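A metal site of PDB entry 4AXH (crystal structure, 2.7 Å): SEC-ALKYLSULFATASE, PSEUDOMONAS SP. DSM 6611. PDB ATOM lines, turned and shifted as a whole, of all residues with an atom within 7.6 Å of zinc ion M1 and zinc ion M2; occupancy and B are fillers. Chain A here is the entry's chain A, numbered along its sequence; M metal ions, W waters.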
ATOM      1  N   ASP A 131       2.956 -19.447 -11.265  1.00  0.00           N
ATOM      2  CA  ASP A 131       1.915 -19.574 -10.221  1.00  0.00           C
ATOM      3  C   ASP A 131       1.717 -21.068  -9.896  1.00  0.00           C
ATOM      4  O   ASP A 131       1.997 -21.917 -10.759  1.00  0.00           O
ATOM      5  CB  ASP A 131       0.577 -19.073 -10.866  1.00  0.00           C
ATOM      6  CG  ASP A 131      -0.650 -18.916  -9.972  1.00  0.00           C
ATOM      7  OD1 ASP A 131      -0.849 -17.806  -9.424  1.00  0.00           O
ATOM      8  OD2 ASP A 131      -1.451 -19.862  -9.910  1.00  0.00           O
ATOM      9  N   PRO A 132       1.094 -21.432  -8.728  1.00  0.00           N
ATOM     10  CA  PRO A 132       0.744 -22.832  -8.511  1.00  0.00           C
ATOM     11  C   PRO A 132      -0.042 -23.484  -9.680  1.00  0.00           C
ATOM     12  O   PRO A 132       0.121 -24.665  -9.952  1.00  0.00           O
ATOM     13  CB  PRO A 132      -0.132 -22.753  -7.248  1.00  0.00           C
ATOM     14  CG  PRO A 132       0.400 -21.611  -6.501  1.00  0.00           C
ATOM     15  CD  PRO A 132       0.696 -20.615  -7.552  1.00  0.00           C
ATOM     16  N   ALA A 133      -0.878 -22.715 -10.378  1.00  0.00           N
ATOM     17  CA  ALA A 133      -1.676 -23.226 -11.496  1.00  0.00           C
ATOM     18  C   ALA A 133      -1.216 -22.713 -12.884  1.00  0.00           C
ATOM     19  O   ALA A 133      -0.225 -21.980 -12.976  1.00  0.00           O
ATOM     20  CB  ALA A 133      -3.144 -22.939 -11.265  1.00  0.00           C
ATOM     21  N   ASN A 134      -1.894 -23.143 -13.946  1.00  0.00           N
ATOM     22  CA  ASN A 134      -1.634 -22.770 -15.334  1.00  0.00           C
ATOM     23  C   ASN A 134      -2.789 -21.960 -15.887  1.00  0.00           C
ATOM     24  O   ASN A 134      -3.946 -22.105 -15.435  1.00  0.00           O
ATOM     25  CB  ASN A 134      -1.457 -24.035 -16.226  1.00  0.00           C
ATOM     26  CG  ASN A 134      -0.424 -25.037 -15.771  1.00  0.00           C
ATOM     27  OD1 ASN A 134       0.524 -24.738 -15.017  1.00  0.00           O
ATOM     28  ND2 ASN A 134      -0.577 -26.249 -16.255  1.00  0.00           N
ATOM     29  N   ASP A 148      -8.976 -20.271 -16.994  1.00  0.00           N
ATOM     30  CA  ASP A 148      -8.450 -19.909 -15.686  1.00  0.00           C
ATOM     31  C   ASP A 148      -7.660 -18.618 -15.641  1.00  0.00           C
ATOM     32  O   ASP A 148      -7.181 -18.120 -16.669  1.00  0.00           O
ATOM     33  CB  ASP A 148      -7.828 -21.095 -14.926  1.00  0.00           C
ATOM     34  CG  ASP A 148      -8.851 -22.168 -14.623  1.00  0.00           C
ATOM     35  OD1 ASP A 148     -10.050 -21.864 -14.667  1.00  0.00           O
ATOM     36  OD2 ASP A 148      -8.449 -23.317 -14.371  1.00  0.00           O
ATOM     37  N   THR A 151      -3.869 -17.828  -9.378  1.00  0.00           N
ATOM     38  CA  THR A 151      -4.193 -17.622  -7.959  1.00  0.00           C
ATOM     39  C   THR A 151      -4.291 -16.160  -7.556  1.00  0.00           C
ATOM     40  O   THR A 151      -5.067 -15.812  -6.665  1.00  0.00           O
ATOM     41  CB  THR A 151      -3.095 -18.305  -7.077  1.00  0.00           C
ATOM     42  OG1 THR A 151      -2.734 -19.555  -7.629  1.00  0.00           O
ATOM     43  CG2 THR A 151      -3.533 -18.522  -5.668  1.00  0.00           C
ATOM     44  N   SER A 178     -12.472 -23.243 -14.714  1.00  0.00           N
ATOM     45  CA  SER A 178     -12.570 -24.703 -14.756  1.00  0.00           C
ATOM     46  C   SER A 178     -13.336 -25.257 -13.529  1.00  0.00           C
ATOM     47  O   SER A 178     -14.140 -26.180 -13.680  1.00  0.00           O
ATOM     48  CB  SER A 178     -11.195 -25.350 -14.850  1.00  0.00           C
ATOM     49  OG  SER A 178     -10.394 -25.146 -13.699  1.00  0.00           O
ATOM     50  N   HIS A 179     -13.065 -24.692 -12.345  1.00  0.00           N
ATOM     51  CA  HIS A 179     -13.661 -25.125 -11.083  1.00  0.00           C
ATOM     52  C   HIS A 179     -13.534 -24.049  -9.976  1.00  0.00           C
ATOM     53  O   HIS A 179     -12.801 -23.058 -10.152  1.00  0.00           O
ATOM     54  CB  HIS A 179     -13.075 -26.497 -10.609  1.00  0.00           C
ATOM     55  CG  HIS A 179     -11.602 -26.491 -10.333  1.00  0.00           C
ATOM     56  ND1 HIS A 179     -10.677 -26.327 -11.357  1.00  0.00           N
ATOM     57  CD2 HIS A 179     -10.939 -26.688  -9.176  1.00  0.00           C
ATOM     58  CE1 HIS A 179      -9.493 -26.430 -10.782  1.00  0.00           C
ATOM     59  NE2 HIS A 179      -9.597 -26.643  -9.463  1.00  0.00           N
ATOM     60  N   SER A 180     -14.219 -24.300  -8.848  1.00  0.00           N
ATOM     61  CA  SER A 180     -14.276 -23.410  -7.688  1.00  0.00           C
ATOM     62  C   SER A 180     -13.029 -23.375  -6.762  1.00  0.00           C
ATOM     63  O   SER A 180     -13.209 -23.286  -5.552  1.00  0.00           O
ATOM     64  CB  SER A 180     -15.567 -23.648  -6.907  1.00  0.00           C
ATOM     65  OG  SER A 180     -15.624 -24.982  -6.450  1.00  0.00           O
ATOM     66  N   HIS A 181     -11.788 -23.383  -7.314  1.00  0.00           N
ATOM     67  CA  HIS A 181     -10.583 -23.263  -6.476  1.00  0.00           C
ATOM     68  C   HIS A 181      -9.860 -21.949  -6.717  1.00  0.00           C
ATOM     69  O   HIS A 181      -9.783 -21.486  -7.852  1.00  0.00           O
ATOM     70  CB  HIS A 181      -9.635 -24.456  -6.621  1.00  0.00           C
ATOM     71  CG  HIS A 181     -10.122 -25.719  -5.989  1.00  0.00           C
ATOM     72  ND1 HIS A 181      -9.712 -26.955  -6.450  1.00  0.00           N
ATOM     73  CD2 HIS A 181     -10.997 -25.907  -4.976  1.00  0.00           C
ATOM     74  CE1 HIS A 181     -10.355 -27.848  -5.695  1.00  0.00           C
ATOM     75  NE2 HIS A 181     -11.116 -27.261  -4.776  1.00  0.00           N
ATOM     76  N   ILE A 182      -9.350 -21.329  -5.630  1.00  0.00           N
ATOM     77  CA  ILE A 182      -8.685 -20.025  -5.679  1.00  0.00           C
ATOM     78  C   ILE A 182      -7.525 -19.910  -6.671  1.00  0.00           C
ATOM     79  O   ILE A 182      -7.282 -18.823  -7.200  1.00  0.00           O
ATOM     80  CB  ILE A 182      -8.351 -19.431  -4.280  1.00  0.00           C
ATOM     81  CG1 ILE A 182      -9.275 -19.988  -3.173  1.00  0.00           C
ATOM     82  CG2 ILE A 182      -8.425 -17.890  -4.319  1.00  0.00           C
ATOM     83  CD1 ILE A 182      -8.739 -19.891  -1.656  1.00  0.00           C
ATOM     84  N   ASP A 183      -6.858 -21.016  -6.979  1.00  0.00           N
ATOM     85  CA  ASP A 183      -5.744 -21.027  -7.931  1.00  0.00           C
ATOM     86  C   ASP A 183      -6.245 -20.981  -9.377  1.00  0.00           C
ATOM     87  O   ASP A 183      -5.448 -20.966 -10.326  1.00  0.00           O
ATOM     88  CB  ASP A 183      -4.775 -22.214  -7.686  1.00  0.00           C
ATOM     89  CG  ASP A 183      -5.385 -23.594  -7.456  1.00  0.00           C
ATOM     90  OD1 ASP A 183      -6.477 -23.686  -6.827  1.00  0.00           O
ATOM     91  OD2 ASP A 183      -4.763 -24.594  -7.861  1.00  0.00           O
ATOM     92  N   HIS A 184      -7.566 -20.911  -9.541  1.00  0.00           N
ATOM     93  CA  HIS A 184      -8.173 -20.897 -10.855  1.00  0.00           C
ATOM     94  C   HIS A 184      -8.981 -19.635 -11.159  1.00  0.00           C
ATOM     95  O   HIS A 184      -9.025 -19.224 -12.328  1.00  0.00           O
ATOM     96  CB  HIS A 184      -8.903 -22.219 -11.124  1.00  0.00           C
ATOM     97  CG  HIS A 184      -7.984 -23.390 -11.030  1.00  0.00           C
ATOM     98  ND1 HIS A 184      -7.263 -23.825 -12.126  1.00  0.00           N
ATOM     99  CD2 HIS A 184      -7.625 -24.113  -9.952  1.00  0.00           C
ATOM    100  CE1 HIS A 184      -6.485 -24.806 -11.688  1.00  0.00           C
ATOM    101  NE2 HIS A 184      -6.680 -25.032 -10.387  1.00  0.00           N
ATOM    102  N   LEU A 249       2.355 -30.584  -7.464  1.00  0.00           N
ATOM    103  CA  LEU A 249       1.665 -30.043  -8.629  1.00  0.00           C
ATOM    104  C   LEU A 249       2.118 -28.645  -9.010  1.00  0.00           C
ATOM    105  O   LEU A 249       1.586 -28.048  -9.950  1.00  0.00           O
ATOM    106  CB  LEU A 249       0.139 -30.070  -8.426  1.00  0.00           C
ATOM    107  CG  LEU A 249      -0.483 -31.423  -8.126  1.00  0.00           C
ATOM    108  CD1 LEU A 249      -1.941 -31.242  -7.763  1.00  0.00           C
ATOM    109  CD2 LEU A 249      -0.320 -32.371  -9.298  1.00  0.00           C
ATOM    110  N   PHE A 250       3.083 -28.106  -8.237  1.00  0.00           N
ATOM    111  CA  PHE A 250       3.712 -26.781  -8.394  1.00  0.00           C
ATOM    112  C   PHE A 250       4.884 -26.662  -7.460  1.00  0.00           C
ATOM    113  O   PHE A 250       5.147 -27.600  -6.710  1.00  0.00           O
ATOM    114  CB  PHE A 250       2.720 -25.625  -8.146  1.00  0.00           C
ATOM    115  CG  PHE A 250       1.785 -25.829  -6.972  1.00  0.00           C
ATOM    116  CD1 PHE A 250       2.183 -25.498  -5.689  1.00  0.00           C
ATOM    117  CD2 PHE A 250       0.522 -26.394  -7.160  1.00  0.00           C
ATOM    118  CE1 PHE A 250       1.361 -25.764  -4.607  1.00  0.00           C
ATOM    119  CE2 PHE A 250      -0.305 -26.639  -6.079  1.00  0.00           C
ATOM    120  CZ  PHE A 250       0.127 -26.332  -4.800  1.00  0.00           C
ATOM    121  N   GLU A 291     -12.570 -33.591  -7.912  1.00  0.00           N
ATOM    122  CA  GLU A 291     -11.490 -32.798  -7.325  1.00  0.00           C
ATOM    123  C   GLU A 291     -12.043 -31.495  -6.645  1.00  0.00           C
ATOM    124  O   GLU A 291     -11.422 -30.985  -5.703  1.00  0.00           O
ATOM    125  CB  GLU A 291     -10.445 -32.479  -8.415  1.00  0.00           C
ATOM    126  CG  GLU A 291      -9.204 -31.782  -7.892  1.00  0.00           C
ATOM    127  CD  GLU A 291      -9.263 -30.276  -7.990  1.00  0.00           C
ATOM    128  OE1 GLU A 291     -10.180 -29.771  -8.689  1.00  0.00           O
ATOM    129  OE2 GLU A 291      -8.369 -29.602  -7.431  1.00  0.00           O
ATOM    130  N   ALA A 292     -13.174 -30.945  -7.139  1.00  0.00           N
ATOM    131  CA  ALA A 292     -13.823 -29.742  -6.611  1.00  0.00           C
ATOM    132  C   ALA A 292     -15.332 -29.895  -6.683  1.00  0.00           C
ATOM    133  O   ALA A 292     -15.815 -30.574  -7.593  1.00  0.00           O
ATOM    134  CB  ALA A 292     -13.399 -28.511  -7.389  1.00  0.00           C
ATOM    135  N   ASP A 295     -17.108 -28.150 -10.699  1.00  0.00           N
ATOM    136  CA  ASP A 295     -15.982 -28.606 -11.537  1.00  0.00           C
ATOM    137  C   ASP A 295     -16.415 -29.058 -12.921  1.00  0.00           C
ATOM    138  O   ASP A 295     -17.532 -29.514 -13.109  1.00  0.00           O
ATOM    139  CB  ASP A 295     -15.331 -29.795 -10.781  1.00  0.00           C
ATOM    140  CG  ASP A 295     -14.007 -30.337 -11.249  1.00  0.00           C
ATOM    141  OD1 ASP A 295     -13.256 -29.578 -11.905  1.00  0.00           O
ATOM    142  OD2 ASP A 295     -13.706 -31.496 -10.924  1.00  0.00           O
ATOM    143  N   ALA A 309      -8.872 -29.810 -16.331  1.00  0.00           N
ATOM    144  CA  ALA A 309      -8.758 -28.970 -15.141  1.00  0.00           C
ATOM    145  C   ALA A 309      -7.713 -29.637 -14.198  1.00  0.00           C
ATOM    146  O   ALA A 309      -6.590 -29.887 -14.655  1.00  0.00           O
ATOM    147  CB  ALA A 309     -10.120 -28.837 -14.466  1.00  0.00           C
ATOM    148  N   ASP A 310      -8.105 -29.966 -12.936  1.00  0.00           N
ATOM    149  CA  ASP A 310      -7.294 -30.660 -11.915  1.00  0.00           C
ATOM    150  C   ASP A 310      -7.799 -32.092 -11.656  1.00  0.00           C
ATOM    151  O   ASP A 310      -7.437 -32.714 -10.626  1.00  0.00           O
ATOM    152  CB  ASP A 310      -7.317 -29.914 -10.579  1.00  0.00           C
ATOM    153  CG  ASP A 310      -6.842 -28.489 -10.599  1.00  0.00           C
ATOM    154  OD1 ASP A 310      -6.467 -28.009 -11.699  1.00  0.00           O
ATOM    155  OD2 ASP A 310      -6.834 -27.856  -9.525  1.00  0.00           O
ATOM    156  N   ASN A 311      -8.661 -32.604 -12.582  1.00  0.00           N
ATOM    157  CA  ASN A 311      -9.272 -33.908 -12.472  1.00  0.00           C
ATOM    158  C   ASN A 311      -8.346 -35.089 -12.693  1.00  0.00           C
ATOM    159  O   ASN A 311      -8.652 -36.197 -12.226  1.00  0.00           O
ATOM    160  CB  ASN A 311     -10.484 -33.989 -13.372  1.00  0.00           C
ATOM    161  CG  ASN A 311     -11.499 -32.978 -12.989  1.00  0.00           C
ATOM    162  OD1 ASN A 311     -11.842 -32.847 -11.808  1.00  0.00           O
ATOM    163  ND2 ASN A 311     -11.907 -32.177 -13.952  1.00  0.00           N
ATOM    164  N   HIS A 317      -3.744 -37.204  -6.611  1.00  0.00           N
ATOM    165  CA  HIS A 317      -4.325 -36.018  -5.949  1.00  0.00           C
ATOM    166  C   HIS A 317      -4.827 -36.422  -4.557  1.00  0.00           C
ATOM    167  O   HIS A 317      -4.707 -37.603  -4.165  1.00  0.00           O
ATOM    168  CB  HIS A 317      -5.434 -35.392  -6.803  1.00  0.00           C
ATOM    169  CG  HIS A 317      -5.561 -33.894  -6.731  1.00  0.00           C
ATOM    170  ND1 HIS A 317      -5.466 -33.210  -5.517  1.00  0.00           N
ATOM    171  CD2 HIS A 317      -5.842 -33.003  -7.719  1.00  0.00           C
ATOM    172  CE1 HIS A 317      -5.677 -31.933  -5.801  1.00  0.00           C
ATOM    173  NE2 HIS A 317      -5.909 -31.750  -7.113  1.00  0.00           N
ATOM    174  N   ARG A 328     -13.319 -36.455  -0.334  1.00  0.00           N
ATOM    175  CA  ARG A 328     -13.789 -36.492  -1.715  1.00  0.00           C
ATOM    176  C   ARG A 328     -14.220 -37.905  -2.083  1.00  0.00           C
ATOM    177  O   ARG A 328     -13.895 -38.861  -1.362  1.00  0.00           O
ATOM    178  CB  ARG A 328     -12.687 -35.976  -2.667  1.00  0.00           C
ATOM    179  CG  ARG A 328     -12.497 -34.520  -2.537  1.00  0.00           C
ATOM    180  CD  ARG A 328     -11.103 -34.150  -2.878  1.00  0.00           C
ATOM    181  NE  ARG A 328     -10.949 -32.694  -3.019  1.00  0.00           N
ATOM    182  CZ  ARG A 328      -9.775 -32.074  -3.141  1.00  0.00           C
ATOM    183  NH1 ARG A 328      -8.638 -32.790  -3.149  1.00  0.00           N
ATOM    184  NH2 ARG A 328      -9.720 -30.747  -3.243  1.00  0.00           N
ATOM    185  N   GLN A 354      -4.561 -27.810 -15.866  1.00  0.00           N
ATOM    186  CA  GLN A 354      -4.408 -26.535 -15.187  1.00  0.00           C
ATOM    187  C   GLN A 354      -3.330 -26.579 -14.091  1.00  0.00           C
ATOM    188  O   GLN A 354      -3.114 -25.632 -13.327  1.00  0.00           O
ATOM    189  CB  GLN A 354      -5.769 -25.974 -14.746  1.00  0.00           C
ATOM    190  CG  GLN A 354      -6.759 -25.815 -15.915  1.00  0.00           C
ATOM    191  CD  GLN A 354      -6.282 -24.778 -16.911  1.00  0.00           C
ATOM    192  OE1 GLN A 354      -5.669 -25.072 -17.943  1.00  0.00           O
ATOM    193  NE2 GLN A 354      -6.555 -23.531 -16.638  1.00  0.00           N
ATOM    194  N   HIS A 355      -2.613 -27.689 -14.044  1.00  0.00           N
ATOM    195  CA  HIS A 355      -1.431 -27.921 -13.248  1.00  0.00           C
ATOM    196  C   HIS A 355      -0.612 -28.805 -14.113  1.00  0.00           C
ATOM    197  O   HIS A 355      -1.166 -29.725 -14.716  1.00  0.00           O
ATOM    198  CB  HIS A 355      -1.737 -28.628 -11.928  1.00  0.00           C
ATOM    199  CG  HIS A 355      -2.385 -27.741 -10.930  1.00  0.00           C
ATOM    200  ND1 HIS A 355      -1.720 -26.695 -10.364  1.00  0.00           N
ATOM    201  CD2 HIS A 355      -3.640 -27.780 -10.443  1.00  0.00           C
ATOM    202  CE1 HIS A 355      -2.573 -26.132  -9.543  1.00  0.00           C
ATOM    203  NE2 HIS A 355      -3.752 -26.761  -9.554  1.00  0.00           N
ATOM    204  N   TYR A 417       1.573 -35.486  -4.417  1.00  0.00           N
ATOM    205  CA  TYR A 417       0.665 -34.505  -3.842  1.00  0.00           C
ATOM    206  C   TYR A 417      -0.200 -35.240  -2.871  1.00  0.00           C
ATOM    207  O   TYR A 417      -0.020 -35.087  -1.663  1.00  0.00           O
ATOM    208  CB  TYR A 417      -0.177 -33.848  -4.951  1.00  0.00           C
ATOM    209  CG  TYR A 417      -0.772 -32.524  -4.542  1.00  0.00           C
ATOM    210  CD1 TYR A 417       0.022 -31.392  -4.439  1.00  0.00           C
ATOM    211  CD2 TYR A 417      -2.145 -32.380  -4.307  1.00  0.00           C
ATOM    212  CE1 TYR A 417      -0.515 -30.156  -4.073  1.00  0.00           C
ATOM    213  CE2 TYR A 417      -2.691 -31.165  -3.943  1.00  0.00           C
ATOM    214  CZ  TYR A 417      -1.876 -30.050  -3.806  1.00  0.00           C
ATOM    215  OH  TYR A 417      -2.388 -28.831  -3.425  1.00  0.00           O
HETATM  216 ZN    ZN M   1      -5.586 -26.162  -9.110  1.00  0.00          ZN
HETATM  217 ZN    ZN M   2      -8.382 -27.520  -8.015  1.00  0.00          ZN
HETATM  218  O   HOH W   1      -6.773 -26.346  -7.382  1.00  0.00           O
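Zinc ion M1 is bound by NE2 of His 355 (2.0 Å). NE2 of His 184 binds zinc ion M1, at 2.0 Å. Water W1 binds zinc ion M1, 2.1 Å away. Zinc ion M1 is bound by OD2 of Asp 310 (2.1 Å). OD2 of Asp 183 binds zinc ion M1, 2.2 Å away.
A ring nitrogen (ND1) of His 355 is in hydrogen-bond range of the backbone carbonyl oxygen (O) of Pro 132 (2.8 Å). ND2 of Asn 134 lies close to N of His 355. A ring nitrogen (ND1) of His 184 lies within hydrogen-bond range of the side-chain carboxylate (OD2) of Asp 148. ND1 of His 179 sits at hydrogen-bond distance from OG of Ser 178 (2.6 Å). The side-chain carboxylate (OE2) of Glu 291 sits close to a ring nitrogen (NE2) of His 317. The backbone carbonyl oxygen of Glu 291 lies within hydrogen-bond range of the guanidinium group of Arg 328.
Five residues have an atom within 4 Å of zinc ion M2: His 179, His 181, His 184, Glu 291 and Asp 310. The nearest printed residue that does not touch zinc ion M2 is Asp 183 (4.4 Å).
Within 4 Å of zinc ion M1: Asp 183, His 184, Asp 310 and His 355. The nearest printed residue that does not touch zinc ion M1 is His 179 (4.1 Å).
Zinc ion M2 is bound by a ring nitrogen (NE2) of His 179 (2.1 Å), water W1 (2.1 Å), a ring nitrogen (ND1) of His 181 (2.1 Å), the side-chain carboxylate (OE2) of Glu 291 (2.2 Å) and the side-chain carboxylate (OD2) of Asp 310 (2.2 Å).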
